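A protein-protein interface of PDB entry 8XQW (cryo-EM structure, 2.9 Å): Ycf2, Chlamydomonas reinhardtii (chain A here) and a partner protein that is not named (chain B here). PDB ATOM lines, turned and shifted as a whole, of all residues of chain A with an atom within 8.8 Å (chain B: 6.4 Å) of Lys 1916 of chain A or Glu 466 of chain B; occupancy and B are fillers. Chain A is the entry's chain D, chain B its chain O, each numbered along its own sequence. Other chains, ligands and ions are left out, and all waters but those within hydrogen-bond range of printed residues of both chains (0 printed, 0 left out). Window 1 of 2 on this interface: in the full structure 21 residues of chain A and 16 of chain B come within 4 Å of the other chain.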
ATOM      1  N   GLN A 328     -38.540 -15.391 -11.641  1.00  0.00           N
ATOM      2  CA  GLN A 328     -38.301 -13.958 -11.601  1.00  0.00           C
ATOM      3  C   GLN A 328     -37.020 -13.573 -12.313  1.00  0.00           C
ATOM      4  O   GLN A 328     -36.845 -12.404 -12.662  1.00  0.00           O
ATOM      5  CB  GLN A 328     -38.250 -13.475 -10.153  1.00  0.00           C
ATOM      6  CG  GLN A 328     -38.356 -11.967  -9.988  1.00  0.00           C
ATOM      7  CD  GLN A 328     -39.513 -11.368 -10.760  1.00  0.00           C
ATOM      8  OE1 GLN A 328     -40.615 -11.907 -10.768  1.00  0.00           O
ATOM      9  NE2 GLN A 328     -39.264 -10.245 -11.415  1.00  0.00           N
ATOM     10  N   LYS A 329     -36.133 -14.531 -12.550  1.00  0.00           N
ATOM     11  CA  LYS A 329     -34.853 -14.270 -13.188  1.00  0.00           C
ATOM     12  C   LYS A 329     -34.895 -14.502 -14.691  1.00  0.00           C
ATOM     13  O   LYS A 329     -34.600 -13.593 -15.465  1.00  0.00           O
ATOM     14  CB  LYS A 329     -33.783 -15.153 -12.552  1.00  0.00           C
ATOM     15  CG  LYS A 329     -32.439 -14.511 -12.412  1.00  0.00           C
ATOM     16  CD  LYS A 329     -31.751 -15.013 -11.169  1.00  0.00           C
ATOM     17  CE  LYS A 329     -30.252 -14.845 -11.261  1.00  0.00           C
ATOM     18  NZ  LYS A 329     -29.866 -13.436 -11.523  1.00  0.00           N
ATOM     19  N   THR A 330     -35.279 -15.701 -15.119  1.00  0.00           N
ATOM     20  CA  THR A 330     -35.208 -16.070 -16.526  1.00  0.00           C
ATOM     21  C   THR A 330     -36.544 -16.589 -17.033  1.00  0.00           C
ATOM     22  O   THR A 330     -37.570 -16.450 -16.368  1.00  0.00           O
ATOM     23  CB  THR A 330     -34.147 -17.144 -16.752  1.00  0.00           C
ATOM     24  OG1 THR A 330     -34.688 -18.418 -16.404  1.00  0.00           O
ATOM     25  CG2 THR A 330     -32.938 -16.894 -15.886  1.00  0.00           C
ATOM     26  N   PHE A 331     -36.532 -17.173 -18.225  1.00  0.00           N
ATOM     27  CA  PHE A 331     -37.693 -17.823 -18.805  1.00  0.00           C
ATOM     28  C   PHE A 331     -37.388 -19.232 -19.278  1.00  0.00           C
ATOM     29  O   PHE A 331     -38.276 -19.884 -19.827  1.00  0.00           O
ATOM     30  CB  PHE A 331     -38.222 -17.016 -19.995  1.00  0.00           C
ATOM     31  CG  PHE A 331     -37.179 -16.765 -21.039  1.00  0.00           C
ATOM     32  CD1 PHE A 331     -36.927 -17.700 -22.026  1.00  0.00           C
ATOM     33  CD2 PHE A 331     -36.419 -15.613 -21.011  1.00  0.00           C
ATOM     34  CE1 PHE A 331     -35.946 -17.483 -22.968  1.00  0.00           C
ATOM     35  CE2 PHE A 331     -35.444 -15.392 -21.956  1.00  0.00           C
ATOM     36  CZ  PHE A 331     -35.207 -16.329 -22.932  1.00  0.00           C
ATOM     37  N   LEU A 332     -36.155 -19.712 -19.102  1.00  0.00           N
ATOM     38  CA  LEU A 332     -35.764 -20.991 -19.682  1.00  0.00           C
ATOM     39  C   LEU A 332     -36.602 -22.140 -19.166  1.00  0.00           C
ATOM     40  O   LEU A 332     -36.785 -23.130 -19.876  1.00  0.00           O
ATOM     41  CB  LEU A 332     -34.299 -21.285 -19.395  1.00  0.00           C
ATOM     42  CG  LEU A 332     -33.260 -20.543 -20.213  1.00  0.00           C
ATOM     43  CD1 LEU A 332     -32.070 -21.441 -20.401  1.00  0.00           C
ATOM     44  CD2 LEU A 332     -33.839 -20.135 -21.545  1.00  0.00           C
ATOM     45  N   SER A1412     -34.758 -13.063 -27.519  1.00  0.00           N
ATOM     46  CA  SER A1412     -33.974 -12.706 -26.342  1.00  0.00           C
ATOM     47  C   SER A1412     -32.479 -12.548 -26.603  1.00  0.00           C
ATOM     48  O   SER A1412     -31.714 -12.494 -25.641  1.00  0.00           O
ATOM     49  CB  SER A1412     -34.153 -13.748 -25.247  1.00  0.00           C
ATOM     50  OG  SER A1412     -33.025 -14.589 -25.196  1.00  0.00           O
ATOM     51  N   SER A1414     -29.461 -10.088 -28.057  1.00  0.00           N
ATOM     52  CA  SER A1414     -29.370  -8.637 -28.207  1.00  0.00           C
ATOM     53  C   SER A1414     -29.333  -8.216 -29.669  1.00  0.00           C
ATOM     54  O   SER A1414     -30.045  -7.286 -30.077  1.00  0.00           O
ATOM     55  CB  SER A1414     -28.137  -8.123 -27.483  1.00  0.00           C
ATOM     56  OG  SER A1414     -27.930  -8.840 -26.287  1.00  0.00           O
ATOM     57  N   ARG A1417     -32.541  -8.025 -31.296  1.00  0.00           N
ATOM     58  CA  ARG A1417     -33.292  -6.825 -30.964  1.00  0.00           C
ATOM     59  C   ARG A1417     -32.812  -5.631 -31.774  1.00  0.00           C
ATOM     60  O   ARG A1417     -33.620  -4.786 -32.169  1.00  0.00           O
ATOM     61  CB  ARG A1417     -33.193  -6.535 -29.477  1.00  0.00           C
ATOM     62  CG  ARG A1417     -33.684  -7.644 -28.619  1.00  0.00           C
ATOM     63  CD  ARG A1417     -33.927  -7.159 -27.234  1.00  0.00           C
ATOM     64  NE  ARG A1417     -33.304  -8.046 -26.271  1.00  0.00           N
ATOM     65  CZ  ARG A1417     -32.210  -7.750 -25.593  1.00  0.00           C
ATOM     66  NH1 ARG A1417     -31.629  -6.579 -25.761  1.00  0.00           N
ATOM     67  NH2 ARG A1417     -31.706  -8.616 -24.737  1.00  0.00           N
ATOM     68  N   SER A1756     -41.878  -7.567 -22.193  1.00  0.00           N
ATOM     69  CA  SER A1756     -40.741  -7.161 -21.381  1.00  0.00           C
ATOM     70  C   SER A1756     -39.436  -7.766 -21.859  1.00  0.00           C
ATOM     71  O   SER A1756     -38.383  -7.421 -21.323  1.00  0.00           O
ATOM     72  CB  SER A1756     -40.954  -7.542 -19.922  1.00  0.00           C
ATOM     73  OG  SER A1756     -40.566  -8.879 -19.694  1.00  0.00           O
ATOM     74  N   THR A1757     -39.478  -8.676 -22.830  1.00  0.00           N
ATOM     75  CA  THR A1757     -38.232  -9.185 -23.385  1.00  0.00           C
ATOM     76  C   THR A1757     -37.742  -8.317 -24.532  1.00  0.00           C
ATOM     77  O   THR A1757     -36.564  -7.958 -24.578  1.00  0.00           O
ATOM     78  CB  THR A1757     -38.399 -10.625 -23.850  1.00  0.00           C
ATOM     79  OG1 THR A1757     -38.607 -11.467 -22.713  1.00  0.00           O
ATOM     80  CG2 THR A1757     -37.159 -11.084 -24.550  1.00  0.00           C
ATOM     81  N   GLN A1760     -35.795  -4.735 -23.921  1.00  0.00           N
ATOM     82  CA  GLN A1760     -34.545  -4.596 -23.205  1.00  0.00           C
ATOM     83  C   GLN A1760     -33.543  -3.846 -24.077  1.00  0.00           C
ATOM     84  O   GLN A1760     -33.696  -3.787 -25.298  1.00  0.00           O
ATOM     85  CB  GLN A1760     -33.988  -5.961 -22.827  1.00  0.00           C
ATOM     86  CG  GLN A1760     -34.936  -6.801 -22.023  1.00  0.00           C
ATOM     87  CD  GLN A1760     -34.235  -7.934 -21.323  1.00  0.00           C
ATOM     88  OE1 GLN A1760     -33.694  -8.835 -21.959  1.00  0.00           O
ATOM     89  NE2 GLN A1760     -34.231  -7.892 -20.002  1.00  0.00           N
ATOM     90  N   ILE A1766     -26.042  -1.625 -24.120  1.00  0.00           N
ATOM     91  CA  ILE A1766     -25.295  -2.409 -23.140  1.00  0.00           C
ATOM     92  C   ILE A1766     -23.814  -2.059 -23.201  1.00  0.00           C
ATOM     93  O   ILE A1766     -23.156  -1.875 -22.167  1.00  0.00           O
ATOM     94  CB  ILE A1766     -25.530  -3.907 -23.375  1.00  0.00           C
ATOM     95  CG1 ILE A1766     -27.020  -4.215 -23.341  1.00  0.00           C
ATOM     96  CG2 ILE A1766     -24.796  -4.723 -22.341  1.00  0.00           C
ATOM     97  CD1 ILE A1766     -27.350  -5.602 -23.798  1.00  0.00           C
ATOM     98  N   ASN A1915     -18.008 -18.289 -11.391  1.00  0.00           N
ATOM     99  CA  ASN A1915     -18.086 -18.049  -9.957  1.00  0.00           C
ATOM    100  C   ASN A1915     -19.325 -17.247  -9.605  1.00  0.00           C
ATOM    101  O   ASN A1915     -19.246 -16.209  -8.951  1.00  0.00           O
ATOM    102  CB  ASN A1915     -16.836 -17.325  -9.468  1.00  0.00           C
ATOM    103  CG  ASN A1915     -15.799 -18.275  -8.927  1.00  0.00           C
ATOM    104  OD1 ASN A1915     -14.606 -18.133  -9.191  1.00  0.00           O
ATOM    105  ND2 ASN A1915     -16.250 -19.265  -8.171  1.00  0.00           N
ATOM    106  N   LYS A1916     -20.477 -17.740 -10.058  1.00  0.00           N
ATOM    107  CA  LYS A1916     -21.741 -17.082  -9.768  1.00  0.00           C
ATOM    108  C   LYS A1916     -22.494 -17.768  -8.641  1.00  0.00           C
ATOM    109  O   LYS A1916     -23.491 -17.227  -8.157  1.00  0.00           O
ATOM    110  CB  LYS A1916     -22.611 -17.057 -11.023  1.00  0.00           C
ATOM    111  CG  LYS A1916     -22.079 -16.175 -12.135  1.00  0.00           C
ATOM    112  CD  LYS A1916     -23.156 -15.889 -13.162  1.00  0.00           C
ATOM    113  CE  LYS A1916     -22.716 -14.818 -14.134  1.00  0.00           C
ATOM    114  NZ  LYS A1916     -23.851 -14.369 -14.975  1.00  0.00           N
ATOM    115  N   ILE A1917     -22.036 -18.943  -8.214  1.00  0.00           N
ATOM    116  CA  ILE A1917     -22.806 -19.820  -7.347  1.00  0.00           C
ATOM    117  C   ILE A1917     -22.029 -20.263  -6.119  1.00  0.00           C
ATOM    118  O   ILE A1917     -22.593 -20.940  -5.256  1.00  0.00           O
ATOM    119  CB  ILE A1917     -23.315 -21.046  -8.132  1.00  0.00           C
ATOM    120  CG1 ILE A1917     -24.568 -21.633  -7.481  1.00  0.00           C
ATOM    121  CG2 ILE A1917     -22.209 -22.074  -8.283  1.00  0.00           C
ATOM    122  CD1 ILE A1917     -25.310 -22.573  -8.375  1.00  0.00           C
ATOM    123  N   LYS A1918     -20.760 -19.893  -6.006  1.00  0.00           N
ATOM    124  CA  LYS A1918     -19.931 -20.258  -4.863  1.00  0.00           C
ATOM    125  C   LYS A1918     -20.435 -19.661  -3.547  1.00  0.00           C
ATOM    126  O   LYS A1918     -20.477 -20.376  -2.536  1.00  0.00           O
ATOM    127  CB  LYS A1918     -18.484 -19.833  -5.113  1.00  0.00           C
ATOM    128  CG  LYS A1918     -17.452 -20.864  -4.703  1.00  0.00           C
ATOM    129  CD  LYS A1918     -16.059 -20.456  -5.162  1.00  0.00           C
ATOM    130  CE  LYS A1918     -15.023 -21.515  -4.824  1.00  0.00           C
ATOM    131  NZ  LYS A1918     -13.783 -21.371  -5.640  1.00  0.00           N
ATOM    132  N   PRO A1919     -20.818 -18.377  -3.498  1.00  0.00           N
ATOM    133  CA  PRO A1919     -21.243 -17.799  -2.212  1.00  0.00           C
ATOM    134  C   PRO A1919     -22.359 -18.559  -1.522  1.00  0.00           C
ATOM    135  O   PRO A1919     -22.377 -18.613  -0.287  1.00  0.00           O
ATOM    136  CB  PRO A1919     -21.692 -16.382  -2.597  1.00  0.00           C
ATOM    137  CG  PRO A1919     -21.834 -16.399  -4.070  1.00  0.00           C
ATOM    138  CD  PRO A1919     -20.801 -17.343  -4.544  1.00  0.00           C
ATOM    139  N   TYR A1920     -23.284 -19.158  -2.272  1.00  0.00           N
ATOM    140  CA  TYR A1920     -24.368 -19.899  -1.639  1.00  0.00           C
ATOM    141  C   TYR A1920     -23.880 -21.157  -0.941  1.00  0.00           C
ATOM    142  O   TYR A1920     -24.610 -21.708  -0.115  1.00  0.00           O
ATOM    143  CB  TYR A1920     -25.433 -20.265  -2.665  1.00  0.00           C
ATOM    144  CG  TYR A1920     -26.037 -19.087  -3.379  1.00  0.00           C
ATOM    145  CD1 TYR A1920     -27.137 -18.426  -2.863  1.00  0.00           C
ATOM    146  CD2 TYR A1920     -25.512 -18.641  -4.578  1.00  0.00           C
ATOM    147  CE1 TYR A1920     -27.690 -17.353  -3.519  1.00  0.00           C
ATOM    148  CE2 TYR A1920     -26.059 -17.572  -5.239  1.00  0.00           C
ATOM    149  CZ  TYR A1920     -27.148 -16.933  -4.708  1.00  0.00           C
ATOM    150  OH  TYR A1920     -27.690 -15.862  -5.373  1.00  0.00           O
ATOM    151  N   PHE A1921     -22.679 -21.631  -1.259  1.00  0.00           N
ATOM    152  CA  PHE A1921     -22.101 -22.763  -0.549  1.00  0.00           C
ATOM    153  C   PHE A1921     -21.120 -22.323   0.528  1.00  0.00           C
ATOM    154  O   PHE A1921     -20.986 -23.000   1.561  1.00  0.00           O
ATOM    155  CB  PHE A1921     -21.412 -23.700  -1.538  1.00  0.00           C
ATOM    156  CG  PHE A1921     -22.356 -24.351  -2.508  1.00  0.00           C
ATOM    157  CD1 PHE A1921     -22.717 -23.712  -3.676  1.00  0.00           C
ATOM    158  CD2 PHE A1921     -22.886 -25.599  -2.247  1.00  0.00           C
ATOM    159  CE1 PHE A1921     -23.582 -24.307  -4.566  1.00  0.00           C
ATOM    160  CE2 PHE A1921     -23.752 -26.195  -3.134  1.00  0.00           C
ATOM    161  CZ  PHE A1921     -24.101 -25.547  -4.293  1.00  0.00           C
ATOM    162  N   GLU A1922     -20.432 -21.200   0.305  1.00  0.00           N
ATOM    163  CA  GLU A1922     -19.599 -20.632   1.360  1.00  0.00           C
ATOM    164  C   GLU A1922     -20.447 -20.177   2.536  1.00  0.00           C
ATOM    165  O   GLU A1922     -19.979 -20.165   3.680  1.00  0.00           O
ATOM    166  CB  GLU A1922     -18.768 -19.467   0.826  1.00  0.00           C
ATOM    167  CG  GLU A1922     -17.314 -19.808   0.556  1.00  0.00           C
ATOM    168  CD  GLU A1922     -17.122 -20.548  -0.745  1.00  0.00           C
ATOM    169  OE1 GLU A1922     -17.937 -20.343  -1.662  1.00  0.00           O
ATOM    170  OE2 GLU A1922     -16.151 -21.321  -0.861  1.00  0.00           O
ATOM    171  N   MET B 452     -22.370 -24.872 -14.213  1.00  0.00           N
ATOM    172  CA  MET B 452     -22.546 -23.488 -14.641  1.00  0.00           C
ATOM    173  C   MET B 452     -21.698 -23.180 -15.867  1.00  0.00           C
ATOM    174  O   MET B 452     -22.171 -22.550 -16.820  1.00  0.00           O
ATOM    175  CB  MET B 452     -22.204 -22.539 -13.502  1.00  0.00           C
ATOM    176  CG  MET B 452     -23.257 -22.494 -12.424  1.00  0.00           C
ATOM    177  SD  MET B 452     -24.650 -21.455 -12.863  1.00  0.00           S
ATOM    178  CE  MET B 452     -25.911 -22.692 -13.069  1.00  0.00           C
ATOM    179  N   LYS B 461     -26.234 -18.847 -23.279  1.00  0.00           N
ATOM    180  CA  LYS B 461     -25.418 -17.909 -22.526  1.00  0.00           C
ATOM    181  C   LYS B 461     -26.191 -17.329 -21.357  1.00  0.00           C
ATOM    182  O   LYS B 461     -27.410 -17.190 -21.406  1.00  0.00           O
ATOM    183  CB  LYS B 461     -24.943 -16.785 -23.431  1.00  0.00           C
ATOM    184  CG  LYS B 461     -23.610 -17.043 -24.062  1.00  0.00           C
ATOM    185  CD  LYS B 461     -23.334 -16.047 -25.151  1.00  0.00           C
ATOM    186  CE  LYS B 461     -22.044 -16.396 -25.841  1.00  0.00           C
ATOM    187  NZ  LYS B 461     -21.718 -17.828 -25.620  1.00  0.00           N
ATOM    188  N   PHE B 462     -25.467 -16.989 -20.292  1.00  0.00           N
ATOM    189  CA  PHE B 462     -26.120 -16.418 -19.123  1.00  0.00           C
ATOM    190  C   PHE B 462     -26.482 -14.966 -19.346  1.00  0.00           C
ATOM    191  O   PHE B 462     -27.376 -14.443 -18.678  1.00  0.00           O
ATOM    192  CB  PHE B 462     -25.228 -16.553 -17.898  1.00  0.00           C
ATOM    193  CG  PHE B 462     -25.314 -17.886 -17.252  1.00  0.00           C
ATOM    194  CD1 PHE B 462     -26.536 -18.480 -17.038  1.00  0.00           C
ATOM    195  CD2 PHE B 462     -24.181 -18.557 -16.875  1.00  0.00           C
ATOM    196  CE1 PHE B 462     -26.624 -19.709 -16.455  1.00  0.00           C
ATOM    197  CE2 PHE B 462     -24.264 -19.786 -16.298  1.00  0.00           C
ATOM    198  CZ  PHE B 462     -25.491 -20.365 -16.086  1.00  0.00           C
ATOM    199  N   SER B 463     -25.803 -14.296 -20.270  1.00  0.00           N
ATOM    200  CA  SER B 463     -26.165 -12.926 -20.584  1.00  0.00           C
ATOM    201  C   SER B 463     -27.405 -12.842 -21.451  1.00  0.00           C
ATOM    202  O   SER B 463     -27.985 -11.760 -21.569  1.00  0.00           O
ATOM    203  CB  SER B 463     -25.005 -12.222 -21.275  1.00  0.00           C
ATOM    204  OG  SER B 463     -24.751 -12.800 -22.536  1.00  0.00           O
ATOM    205  N   TRP B 464     -27.822 -13.945 -22.058  1.00  0.00           N
ATOM    206  CA  TRP B 464     -29.045 -13.961 -22.842  1.00  0.00           C
ATOM    207  C   TRP B 464     -30.263 -14.240 -21.987  1.00  0.00           C
ATOM    208  O   TRP B 464     -31.266 -13.534 -22.088  1.00  0.00           O
ATOM    209  CB  TRP B 464     -28.961 -15.020 -23.934  1.00  0.00           C
ATOM    210  CG  TRP B 464     -28.020 -14.703 -25.016  1.00  0.00           C
ATOM    211  CD1 TRP B 464     -27.458 -13.504 -25.277  1.00  0.00           C
ATOM    212  CD2 TRP B 464     -27.526 -15.602 -26.000  1.00  0.00           C
ATOM    213  NE1 TRP B 464     -26.639 -13.596 -26.364  1.00  0.00           N
ATOM    214  CE2 TRP B 464     -26.666 -14.881 -26.827  1.00  0.00           C
ATOM    215  CE3 TRP B 464     -27.730 -16.955 -26.263  1.00  0.00           C
ATOM    216  CZ2 TRP B 464     -26.010 -15.460 -27.890  1.00  0.00           C
ATOM    217  CZ3 TRP B 464     -27.080 -17.526 -27.317  1.00  0.00           C
ATOM    218  CH2 TRP B 464     -26.232 -16.782 -28.120  1.00  0.00           C
ATOM    219  N   SER B 465     -30.189 -15.257 -21.135  1.00  0.00           N
ATOM    220  CA  SER B 465     -31.381 -15.741 -20.458  1.00  0.00           C
ATOM    221  C   SER B 465     -31.785 -14.847 -19.296  1.00  0.00           C
ATOM    222  O   SER B 465     -32.960 -14.803 -18.929  1.00  0.00           O
ATOM    223  CB  SER B 465     -31.157 -17.168 -19.981  1.00  0.00           C
ATOM    224  OG  SER B 465     -29.810 -17.362 -19.618  1.00  0.00           O
ATOM    225  N   GLU B 466     -30.838 -14.138 -18.700  1.00  0.00           N
ATOM    226  CA  GLU B 466     -31.146 -13.267 -17.580  1.00  0.00           C
ATOM    227  C   GLU B 466     -31.506 -11.868 -18.062  1.00  0.00           C
ATOM    228  O   GLU B 466     -31.052 -11.407 -19.107  1.00  0.00           O
ATOM    229  CB  GLU B 466     -29.969 -13.202 -16.616  1.00  0.00           C
ATOM    230  CG  GLU B 466     -29.812 -14.452 -15.784  1.00  0.00           C
ATOM    231  CD  GLU B 466     -28.497 -14.502 -15.039  1.00  0.00           C
ATOM    232  OE1 GLU B 466     -27.565 -13.765 -15.421  1.00  0.00           O
ATOM    233  OE2 GLU B 466     -28.391 -15.284 -14.072  1.00  0.00           O
ATOM    234  N   LYS B 467     -32.331 -11.192 -17.274  1.00  0.00           N
ATOM    235  CA  LYS B 467     -32.802  -9.865 -17.627  1.00  0.00           C
ATOM    236  C   LYS B 467     -31.721  -8.821 -17.388  1.00  0.00           C
ATOM    237  O   LYS B 467     -30.909  -8.934 -16.466  1.00  0.00           O
ATOM    238  CB  LYS B 467     -34.040  -9.505 -16.812  1.00  0.00           C
ATOM    239  CG  LYS B 467     -35.223 -10.404 -17.060  1.00  0.00           C
ATOM    240  CD  LYS B 467     -36.450  -9.895 -16.341  1.00  0.00           C
ATOM    241  CE  LYS B 467     -37.474 -10.992 -16.189  1.00  0.00           C
ATOM    242  NZ  LYS B 467     -38.633 -10.536 -15.385  1.00  0.00           N
ATOM    243  N   THR B 468     -31.719  -7.792 -18.230  1.00  0.00           N
ATOM    244  CA  THR B 468     -30.842  -6.644 -18.067  1.00  0.00           C
ATOM    245  C   THR B 468     -31.654  -5.445 -17.600  1.00  0.00           C
ATOM    246  O   THR B 468     -32.834  -5.308 -17.929  1.00  0.00           O
ATOM    247  CB  THR B 468     -30.115  -6.294 -19.369  1.00  0.00           C
ATOM    248  OG1 THR B 468     -30.963  -5.477 -20.183  1.00  0.00           O
ATOM    249  CG2 THR B 468     -29.757  -7.549 -20.134  1.00  0.00           C
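The side-chain carboxylate of Glu 466 of chain B lies within salt-bridge range of the side-chain amino group of Lys 1916 of chain A (3.8 Å).
The side-chain amide nitrogen (NE2) of Gln 1760 of chain A lies close to the backbone NH (N) of Thr 468 of chain B (3.1 Å).
The side-chain carboxylate of Glu 466 of chain B is in salt-bridge range of the side-chain amino group of Lys 329 of chain A (3.5 Å).
The side-chain hydroxyl (OG) of Ser 465 of chain B sits at hydrogen-bond distance from the backbone carbonyl oxygen (O) of Lys 461 of chain B (3.0 Å).
OE1 of Gln 1760 of chain A sits at hydrogen-bond distance from NH2 of Arg 1417 of chain A (3.4 Å).
The side-chain hydroxyl (OG1) of Thr 330 of chain A is in hydrogen-bond range of the backbone NH (N) of Leu 332 of chain A (3.3 Å).
Among the printed residues, merely in contact across the chains: Gln 328 of chain A with Lys 467 of chain B (3.8 Å), Lys 329 of chain A with Lys 467 of chain B (3.6 Å), Thr 330 of chain A with Ser 465 of chain B (3.4 Å), Thr 330 of chain A with Glu 466 of chain B (3.97 Å), Phe 331 of chain A with Ser 465 of chain B (3.96 Å), Leu 332 of chain A with Ser 465 of chain B (3.98 Å), Ser 1412 of chain A with Trp 464 of chain B (3.7 Å), Gln 1760 of chain A with Lys 467 of chain B (3.4 Å) and Lys 1916 of chain A with Phe 462 of chain B (3.9 Å).
Of chain B, only Phe 462 (3.9 Å) and Glu 466 (3.8 Å) come within 4 Å of Lys 1916 of chain A.
Of chain A, only Lys 329 (3.4 Å), Thr 330 (3.97 Å) and Lys 1916 (3.8 Å) come within 4 Å of Glu 466 of chain B.
Of the printed residues of chain B, Phe 331 of chain A touches Ser 465.
Printed residues of chain A within 4 Å of Phe 462 of chain B: Lys 1916.
Printed residues of chain B within 4 Å of Thr 330 of chain A: Ser 465 and Glu 466.
Of the printed residues of chain B, Leu 332 of chain A touches Ser 465 (3.98 Å).
Of the printed residues of chain B, Ser 1412 of chain A touches Trp 464.
Of the 9 printed residues of chain B, 6 touch a printed residue of chain A.
Printed residues of chain B that touch a printed residue of chain A: Phe 462, Trp 464, Ser 465, Glu 466, Lys 467 and Thr 468.
Hydrophobic or aromatic side chains of chain B within 4 Å of the printed part of chain A: Phe 462.
Among the printed residues, 12 pairs touch across the chains.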
